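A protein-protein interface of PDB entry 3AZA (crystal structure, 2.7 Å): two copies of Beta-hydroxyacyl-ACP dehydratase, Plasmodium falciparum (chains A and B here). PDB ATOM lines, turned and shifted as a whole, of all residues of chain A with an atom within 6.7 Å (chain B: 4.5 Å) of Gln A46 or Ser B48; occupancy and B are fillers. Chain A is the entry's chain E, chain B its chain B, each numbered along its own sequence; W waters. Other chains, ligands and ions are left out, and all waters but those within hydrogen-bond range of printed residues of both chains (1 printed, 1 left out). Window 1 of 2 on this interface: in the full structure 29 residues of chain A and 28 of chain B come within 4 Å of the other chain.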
ATOM      1  N   LEU A  27      20.995  21.901  -0.207  1.00  0.00           N
ATOM      2  CA  LEU A  27      21.284  21.853  -1.630  1.00  0.00           C
ATOM      3  C   LEU A  27      21.191  20.396  -2.027  1.00  0.00           C
ATOM      4  O   LEU A  27      21.981  19.579  -1.557  1.00  0.00           O
ATOM      5  CB  LEU A  27      22.687  22.404  -1.932  1.00  0.00           C
ATOM      6  CG  LEU A  27      23.111  22.528  -3.407  1.00  0.00           C
ATOM      7  CD1 LEU A  27      22.221  23.472  -4.199  1.00  0.00           C
ATOM      8  CD2 LEU A  27      24.578  22.941  -3.512  1.00  0.00           C
ATOM      9  N   LEU A  28      20.225  20.081  -2.887  1.00  0.00           N
ATOM     10  CA  LEU A  28      19.903  18.696  -3.236  1.00  0.00           C
ATOM     11  C   LEU A  28      20.085  18.358  -4.717  1.00  0.00           C
ATOM     12  O   LEU A  28      19.490  17.396  -5.226  1.00  0.00           O
ATOM     13  CB  LEU A  28      18.482  18.363  -2.793  1.00  0.00           C
ATOM     14  CG  LEU A  28      18.206  18.348  -1.288  1.00  0.00           C
ATOM     15  CD1 LEU A  28      16.797  17.837  -1.026  1.00  0.00           C
ATOM     16  CD2 LEU A  28      19.233  17.512  -0.535  1.00  0.00           C
ATOM     17  N   VAL A  29      20.919  19.152  -5.391  1.00  0.00           N
ATOM     18  CA  VAL A  29      21.299  18.928  -6.782  1.00  0.00           C
ATOM     19  C   VAL A  29      22.814  18.847  -6.793  1.00  0.00           C
ATOM     20  O   VAL A  29      23.489  19.821  -6.468  1.00  0.00           O
ATOM     21  CB  VAL A  29      20.836  20.080  -7.706  1.00  0.00           C
ATOM     22  CG1 VAL A  29      21.380  19.898  -9.112  1.00  0.00           C
ATOM     23  CG2 VAL A  29      19.312  20.173  -7.736  1.00  0.00           C
ATOM     24  N   ASP A  30      23.333  17.676  -7.161  1.00  0.00           N
ATOM     25  CA  ASP A  30      24.765  17.417  -7.166  1.00  0.00           C
ATOM     26  C   ASP A  30      25.429  17.811  -8.473  1.00  0.00           C
ATOM     27  O   ASP A  30      26.596  18.194  -8.483  1.00  0.00           O
ATOM     28  CB  ASP A  30      25.027  15.936  -6.922  1.00  0.00           C
ATOM     29  CG  ASP A  30      24.973  15.567  -5.467  1.00  0.00           C
ATOM     30  OD1 ASP A  30      25.434  16.354  -4.621  1.00  0.00           O
ATOM     31  OD2 ASP A  30      24.485  14.464  -5.169  1.00  0.00           O
ATOM     32  N   LEU A  44      21.332  15.093 -11.472  1.00  0.00           N
ATOM     33  CA  LEU A  44      21.448  13.951 -10.588  1.00  0.00           C
ATOM     34  C   LEU A  44      21.809  14.359  -9.165  1.00  0.00           C
ATOM     35  O   LEU A  44      22.478  15.377  -8.939  1.00  0.00           O
ATOM     36  CB  LEU A  44      22.442  12.912 -11.152  1.00  0.00           C
ATOM     37  CG  LEU A  44      23.876  13.332 -11.514  1.00  0.00           C
ATOM     38  CD1 LEU A  44      24.770  13.323 -10.274  1.00  0.00           C
ATOM     39  CD2 LEU A  44      24.460  12.418 -12.586  1.00  0.00           C
ATOM     40  N   LYS A  45      21.333  13.557  -8.216  1.00  0.00           N
ATOM     41  CA  LYS A  45      21.696  13.683  -6.817  1.00  0.00           C
ATOM     42  C   LYS A  45      22.130  12.309  -6.330  1.00  0.00           C
ATOM     43  O   LYS A  45      21.372  11.339  -6.409  1.00  0.00           O
ATOM     44  CB  LYS A  45      20.510  14.218  -5.994  1.00  0.00           C
ATOM     45  CG  LYS A  45      20.834  14.562  -4.533  1.00  0.00           C
ATOM     46  CD  LYS A  45      20.515  13.389  -3.608  1.00  0.00           C
ATOM     47  CE  LYS A  45      20.695  13.749  -2.146  1.00  0.00           C
ATOM     48  NZ  LYS A  45      22.113  14.027  -1.813  1.00  0.00           N
ATOM     49  N   GLN A  46      23.361  12.233  -5.842  1.00  0.00           N
ATOM     50  CA  GLN A  46      23.894  10.996  -5.287  1.00  0.00           C
ATOM     51  C   GLN A  46      23.310  10.744  -3.895  1.00  0.00           C
ATOM     52  O   GLN A  46      23.363  11.621  -3.028  1.00  0.00           O
ATOM     53  CB  GLN A  46      25.425  11.046  -5.248  1.00  0.00           C
ATOM     54  CG  GLN A  46      26.086  11.186  -6.628  1.00  0.00           C
ATOM     55  CD  GLN A  46      25.745  10.034  -7.584  1.00  0.00           C
ATOM     56  OE1 GLN A  46      25.421   8.929  -7.145  1.00  0.00           O
ATOM     57  NE2 GLN A  46      25.815  10.295  -8.893  1.00  0.00           N
ATOM     58  N   VAL A  47      22.737   9.558  -3.692  1.00  0.00           N
ATOM     59  CA  VAL A  47      22.102   9.234  -2.415  1.00  0.00           C
ATOM     60  C   VAL A  47      23.044   8.409  -1.552  1.00  0.00           C
ATOM     61  O   VAL A  47      23.260   7.224  -1.818  1.00  0.00           O
ATOM     62  CB  VAL A  47      20.757   8.479  -2.591  1.00  0.00           C
ATOM     63  CG1 VAL A  47      19.945   8.539  -1.304  1.00  0.00           C
ATOM     64  CG2 VAL A  47      19.949   9.059  -3.751  1.00  0.00           C
ATOM     65  N   SER A  48      23.598   9.046  -0.522  1.00  0.00           N
ATOM     66  CA  SER A  48      24.545   8.396   0.379  1.00  0.00           C
ATOM     67  C   SER A  48      24.012   8.331   1.804  1.00  0.00           C
ATOM     68  O   SER A  48      23.152   9.124   2.188  1.00  0.00           O
ATOM     69  CB  SER A  48      25.879   9.139   0.377  1.00  0.00           C
ATOM     70  OG  SER A  48      26.841   8.421   1.135  1.00  0.00           O
ATOM     71  N   ASN A  50      25.913   8.951   4.304  1.00  0.00           N
ATOM     72  CA  ASN A  50      26.583  10.083   4.929  1.00  0.00           C
ATOM     73  C   ASN A  50      25.884  11.411   4.656  1.00  0.00           C
ATOM     74  O   ASN A  50      26.530  12.416   4.342  1.00  0.00           O
ATOM     75  CB  ASN A  50      28.049  10.163   4.488  1.00  0.00           C
ATOM     76  CG  ASN A  50      28.938  10.743   5.567  1.00  0.00           C
ATOM     77  OD1 ASN A  50      28.744  10.463   6.754  1.00  0.00           O
ATOM     78  ND2 ASN A  50      29.916  11.548   5.172  1.00  0.00           N
ATOM     79  N   GLU A  51      24.560  11.399   4.783  1.00  0.00           N
ATOM     80  CA  GLU A  51      23.749  12.595   4.661  1.00  0.00           C
ATOM     81  C   GLU A  51      22.976  12.788   5.957  1.00  0.00           C
ATOM     82  O   GLU A  51      22.530  11.802   6.558  1.00  0.00           O
ATOM     83  CB  GLU A  51      22.800  12.482   3.472  1.00  0.00           C
ATOM     84  CG  GLU A  51      23.505  12.512   2.137  1.00  0.00           C
ATOM     85  CD  GLU A  51      22.556  12.662   0.976  1.00  0.00           C
ATOM     86  OE1 GLU A  51      21.901  13.719   0.872  1.00  0.00           O
ATOM     87  OE2 GLU A  51      22.474  11.729   0.156  1.00  0.00           O
ATOM     88  N   MET A  64      15.138   7.722   1.745  1.00  0.00           N
ATOM     89  CA  MET A  64      15.189   9.135   1.390  1.00  0.00           C
ATOM     90  C   MET A  64      13.782   9.710   1.471  1.00  0.00           C
ATOM     91  O   MET A  64      12.884   9.239   0.774  1.00  0.00           O
ATOM     92  CB  MET A  64      15.797   9.344  -0.001  1.00  0.00           C
ATOM     93  CG  MET A  64      15.658  10.768  -0.504  1.00  0.00           C
ATOM     94  SD  MET A  64      16.844  11.208  -1.773  1.00  0.00           S
ATOM     95  CE  MET A  64      16.397  12.927  -2.034  1.00  0.00           C
ATOM     96  N   GLY A 110      23.044   4.407  -1.787  1.00  0.00           N
ATOM     97  CA  GLY A 110      23.619   3.597  -2.853  1.00  0.00           C
ATOM     98  C   GLY A 110      23.076   3.957  -4.224  1.00  0.00           C
ATOM     99  O   GLY A 110      23.789   3.836  -5.221  1.00  0.00           O
ATOM    100  N   ASP A 111      21.817   4.401  -4.272  1.00  0.00           N
ATOM    101  CA  ASP A 111      21.161   4.798  -5.520  1.00  0.00           C
ATOM    102  C   ASP A 111      21.763   6.053  -6.157  1.00  0.00           C
ATOM    103  O   ASP A 111      22.487   6.811  -5.511  1.00  0.00           O
ATOM    104  CB  ASP A 111      19.664   5.035  -5.287  1.00  0.00           C
ATOM    105  CG  ASP A 111      18.919   3.784  -4.841  1.00  0.00           C
ATOM    106  OD1 ASP A 111      19.458   2.661  -4.949  1.00  0.00           O
ATOM    107  OD2 ASP A 111      17.767   3.930  -4.384  1.00  0.00           O
ATOM    108  N   THR A 112      21.470   6.248  -7.441  1.00  0.00           N
ATOM    109  CA  THR A 112      21.735   7.505  -8.118  1.00  0.00           C
ATOM    110  C   THR A 112      20.395   8.032  -8.577  1.00  0.00           C
ATOM    111  O   THR A 112      19.685   7.362  -9.356  1.00  0.00           O
ATOM    112  CB  THR A 112      22.637   7.323  -9.339  1.00  0.00           C
ATOM    113  OG1 THR A 112      23.879   6.752  -8.923  1.00  0.00           O
ATOM    114  CG2 THR A 112      22.914   8.667 -10.002  1.00  0.00           C
ATOM    115  N   LEU A 113      20.041   9.219  -8.082  1.00  0.00           N
ATOM    116  CA  LEU A 113      18.778   9.843  -8.439  1.00  0.00           C
ATOM    117  C   LEU A 113      18.968  10.690  -9.693  1.00  0.00           C
ATOM    118  O   LEU A 113      19.592  11.748  -9.644  1.00  0.00           O
ATOM    119  CB  LEU A 113      18.249  10.689  -7.272  1.00  0.00           C
ATOM    120  CG  LEU A 113      16.883  11.380  -7.401  1.00  0.00           C
ATOM    121  CD1 LEU A 113      15.756  10.395  -7.749  1.00  0.00           C
ATOM    122  CD2 LEU A 113      16.559  12.132  -6.122  1.00  0.00           C
ATOM    123  N   GLN B  46      28.293   6.741  -2.650  1.00  0.00           N
ATOM    124  CA  GLN B  46      27.765   7.830  -3.463  1.00  0.00           C
ATOM    125  C   GLN B  46      28.225   9.176  -2.910  1.00  0.00           C
ATOM    126  O   GLN B  46      28.048   9.469  -1.727  1.00  0.00           O
ATOM    127  CB  GLN B  46      26.238   7.761  -3.540  1.00  0.00           C
ATOM    128  CG  GLN B  46      25.678   6.449  -4.120  1.00  0.00           C
ATOM    129  CD  GLN B  46      26.037   6.215  -5.594  1.00  0.00           C
ATOM    130  OE1 GLN B  46      26.600   7.085  -6.264  1.00  0.00           O
ATOM    131  NE2 GLN B  46      25.706   5.035  -6.100  1.00  0.00           N
ATOM    132  N   VAL B  47      28.831   9.982  -3.774  1.00  0.00           N
ATOM    133  CA  VAL B  47      29.452  11.243  -3.385  1.00  0.00           C
ATOM    134  C   VAL B  47      28.488  12.381  -3.687  1.00  0.00           C
ATOM    135  O   VAL B  47      28.300  12.746  -4.850  1.00  0.00           O
ATOM    136  CB  VAL B  47      30.773  11.473  -4.158  1.00  0.00           C
ATOM    137  CG1 VAL B  47      31.692  12.434  -3.401  1.00  0.00           C
ATOM    138  CG2 VAL B  47      31.486  10.149  -4.383  1.00  0.00           C
ATOM    139  N   SER B  48      27.870  12.924  -2.638  1.00  0.00           N
ATOM    140  CA  SER B  48      26.893  13.999  -2.781  1.00  0.00           C
ATOM    141  C   SER B  48      27.377  15.283  -2.131  1.00  0.00           C
ATOM    142  O   SER B  48      28.175  15.241  -1.200  1.00  0.00           O
ATOM    143  CB  SER B  48      25.560  13.593  -2.158  1.00  0.00           C
ATOM    144  OG  SER B  48      24.584  14.601  -2.383  1.00  0.00           O
ATOM    145  N   THR B  49      26.878  16.419  -2.620  1.00  0.00           N
ATOM    146  CA  THR B  49      27.136  17.723  -2.002  1.00  0.00           C
ATOM    147  C   THR B  49      26.509  17.831  -0.604  1.00  0.00           C
ATOM    148  O   THR B  49      26.972  18.603   0.239  1.00  0.00           O
ATOM    149  CB  THR B  49      26.625  18.902  -2.889  1.00  0.00           C
ATOM    150  OG1 THR B  49      27.128  20.140  -2.374  1.00  0.00           O
ATOM    151  CG2 THR B  49      25.089  18.969  -2.934  1.00  0.00           C
ATOM    152  N   ASN B  50      25.461  17.044  -0.371  1.00  0.00           N
ATOM    153  CA  ASN B  50      24.716  17.085   0.875  1.00  0.00           C
ATOM    154  C   ASN B  50      25.378  16.242   1.962  1.00  0.00           C
ATOM    155  O   ASN B  50      24.709  15.541   2.721  1.00  0.00           O
ATOM    156  CB  ASN B  50      23.278  16.635   0.629  1.00  0.00           C
ATOM    157  CG  ASN B  50      22.304  17.223   1.631  1.00  0.00           C
ATOM    158  OD1 ASN B  50      22.448  18.371   2.056  1.00  0.00           O
ATOM    159  ND2 ASN B  50      21.296  16.437   2.008  1.00  0.00           N
ATOM    160  N   GLU B  51      26.707  16.320   2.020  1.00  0.00           N
ATOM    161  CA  GLU B  51      27.499  15.559   2.974  1.00  0.00           C
ATOM    162  C   GLU B  51      28.256  16.541   3.845  1.00  0.00           C
ATOM    163  O   GLU B  51      28.726  17.564   3.343  1.00  0.00           O
ATOM    164  CB  GLU B  51      28.458  14.610   2.255  1.00  0.00           C
ATOM    165  CG  GLU B  51      27.770  13.421   1.603  1.00  0.00           C
ATOM    166  CD  GLU B  51      28.735  12.306   1.249  1.00  0.00           C
ATOM    167  OE1 GLU B  51      29.421  11.789   2.157  1.00  0.00           O
ATOM    168  OE2 GLU B  51      28.797  11.932   0.054  1.00  0.00           O
ATOM    169  N   PHE B  54      31.958  18.380   3.195  1.00  0.00           N
ATOM    170  CA  PHE B  54      32.215  19.164   1.988  1.00  0.00           C
ATOM    171  C   PHE B  54      32.318  20.662   2.249  1.00  0.00           C
ATOM    172  O   PHE B  54      33.117  21.343   1.611  1.00  0.00           O
ATOM    173  CB  PHE B  54      31.178  18.862   0.899  1.00  0.00           C
ATOM    174  CG  PHE B  54      31.569  17.735  -0.022  1.00  0.00           C
ATOM    175  CD1 PHE B  54      32.803  17.738  -0.672  1.00  0.00           C
ATOM    176  CD2 PHE B  54      30.694  16.685  -0.266  1.00  0.00           C
ATOM    177  CE1 PHE B  54      33.165  16.699  -1.544  1.00  0.00           C
ATOM    178  CE2 PHE B  54      31.051  15.642  -1.134  1.00  0.00           C
ATOM    179  CZ  PHE B  54      32.288  15.656  -1.773  1.00  0.00           C
ATOM    180  N   GLY B 110      28.667  14.284  -7.440  1.00  0.00           N
ATOM    181  CA  GLY B 110      28.169  13.768  -8.713  1.00  0.00           C
ATOM    182  C   GLY B 110      28.685  12.384  -9.055  1.00  0.00           C
ATOM    183  O   GLY B 110      28.012  11.621  -9.760  1.00  0.00           O
ATOM    184  N   ASP B 111      29.872  12.054  -8.552  1.00  0.00           N
ATOM    185  CA  ASP B 111      30.504  10.771  -8.851  1.00  0.00           C
ATOM    186  C   ASP B 111      29.850   9.611  -8.105  1.00  0.00           C
ATOM    187  O   ASP B 111      29.137   9.810  -7.112  1.00  0.00           O
ATOM    188  CB  ASP B 111      32.001  10.810  -8.525  1.00  0.00           C
ATOM    189  CG  ASP B 111      32.730  11.939  -9.232  1.00  0.00           C
ATOM    190  OD1 ASP B 111      32.275  12.372 -10.306  1.00  0.00           O
ATOM    191  OD2 ASP B 111      33.771  12.390  -8.714  1.00  0.00           O
ATOM    192  N   THR B 112      30.072   8.407  -8.629  1.00  0.00           N
ATOM    193  CA  THR B 112      29.870   7.174  -7.890  1.00  0.00           C
ATOM    194  C   THR B 112      31.278   6.672  -7.634  1.00  0.00           C
ATOM    195  O   THR B 112      32.133   6.736  -8.525  1.00  0.00           O
ATOM    196  CB  THR B 112      29.076   6.139  -8.711  1.00  0.00           C
ATOM    197  OG1 THR B 112      27.773   6.655  -8.999  1.00  0.00           O
ATOM    198  CG2 THR B 112      28.927   4.829  -7.947  1.00  0.00           C
HETATM  199  O   HOH W   1      24.065  20.473   0.829  1.00  0.00           O
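Water W1 bridges OD1 of Asn B50 (2.9 Å) and O of Leu A27 (3.3 Å).
Leu A27 touches Thr B49 (O to CG2, 3.5 Å).
O of Leu A27 touches OD1 of Asn B50 (3.8 Å).
CD2 of Leu A28 touches ND2 of Asn B50, 3.4 Å away.
Thr B49 touches Val A29 (CG2 to O, 3.97 Å).
Val B47 touches Gln A46 (O to CG, 3.2 Å).
Asp B111 touches Gln A46 (O to CG, 3.4 Å).
Gln A46 touches Thr B112.
Val A47 touches Gln B46.
Asn A50 touches Asn B50 (O to O, 3.96 Å).
Thr A112 touches Gln B46.
The side-chain hydroxyl (OG) of Ser A48 lies close to the backbone carbonyl oxygen (O) of Gln B46.
The side-chain amide nitrogen of Gln B46 is in hydrogen-bond range of the backbone carbonyl oxygen of Gly A110.
OG of Ser B48 sits at hydrogen-bond distance from OD2 of Asp A30 (2.8 Å).
The side-chain hydroxyl (OG) of Ser B48 is in hydrogen-bond range of the side-chain amino group (NZ) of Lys A45.
The side-chain hydroxyl (OG) of Ser B48 sits close to the backbone carbonyl oxygen (O) of Gln A46, 3.3 Å away.
The backbone NH of Thr B49 is in hydrogen-bond range of the side-chain carboxylate of Asp A30, 2.5 Å away.
The side-chain amide nitrogen (ND2) of Asn B50 lies within hydrogen-bond range of the side-chain carboxylate (OE1) of Glu A51 (3.0 Å).
OE1 of Glu B51 sits at hydrogen-bond distance from ND2 of Asn A50 (3.1 Å).
O of Gly B110 lies within hydrogen-bond range of NE2 of Gln A46.
OE1 of Gln B46 sits close to OE1 of Gln A46.
The backbone carbonyl oxygen (O) of Val B47 lies within hydrogen-bond range of the backbone NH (N) of Gly B110, at 3.0 Å.
The backbone carbonyl oxygen of Asp B111 sits at hydrogen-bond distance from the backbone NH of Val B47 (3.4 Å).
OD2 of Asp A30 sits at hydrogen-bond distance from N of Gln A46, 2.6 Å away.
The backbone NH of Val A47 is in hydrogen-bond range of the backbone carbonyl oxygen of Asp A111, at 3.3 Å.
N of Asn A50 lies close to OG of Ser A48.
The side-chain carboxylate of Glu A51 is in hydrogen-bond range of the backbone NH of Ser A48.
Gln A46 touches its own counterpart, Gln B46.
Gln A46 touches Asp B111, and with the chains exchanged Asp A111 touches Gln B46.
Gln A46 touches Thr B112, and with the chains exchanged Thr A112 touches Gln B46.
Asn A50 touches Glu B51, and with the chains exchanged Glu A51 touches Asn B50.
Positions printed for both chains: 46, 47, 48, 50, 51, 110, 111 and 112.
Of the 16 printed residues of chain A, 14 touch a printed residue of chain B.
Printed residues of chain A that touch a printed residue of chain B: Leu A27, Leu A28, Val A29, Asp A30, Leu A44, Lys A45, Gln A46, Val A47, Ser A48, Asn A50, Glu A51, Gly A110, Asp A111 and Thr A112.
Hydrophobic or aromatic side chains of chain A that line the printed part of chain B: Leu A27, Leu A28 and Leu A44.
Among the printed residues, no Asp or Glu carboxylate lies within 4 Å of a Lys or Arg side-chain nitrogen of the other chain.
Gln A46 touches just these residues of chain B: Gln B46 (2.4 Å), Val B47 (3.2 Å), Ser B48 (3.1 Å), Gly B110 (2.7 Å), Asp B111 (3.4 Å) and Thr B112 (3.8 Å).
Ser B48 touches three residues of chain A.
Printed residues of chain B within 4 Å of Ser A48: Gln B46.
Of the printed residues of chain A, Glu B51 touches Asn A50 (3.1 Å).
Of the printed residues of chain B, Leu A27 touches Thr B49 (3.5 Å) and Asn B50 (3.8 Å).
Printed residues of chain B within 4 Å of Glu A51: Asn B50 (3.0 Å).
Of the printed residues of chain A, Thr B112 touches Gln A46 (3.8 Å) and Thr A112 (3.9 Å).
Phe B54 touches none of the printed residues of chain A.
The nearest printed residue of chain A that does not touch Asp B111 is Leu A44 (5.5 Å).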
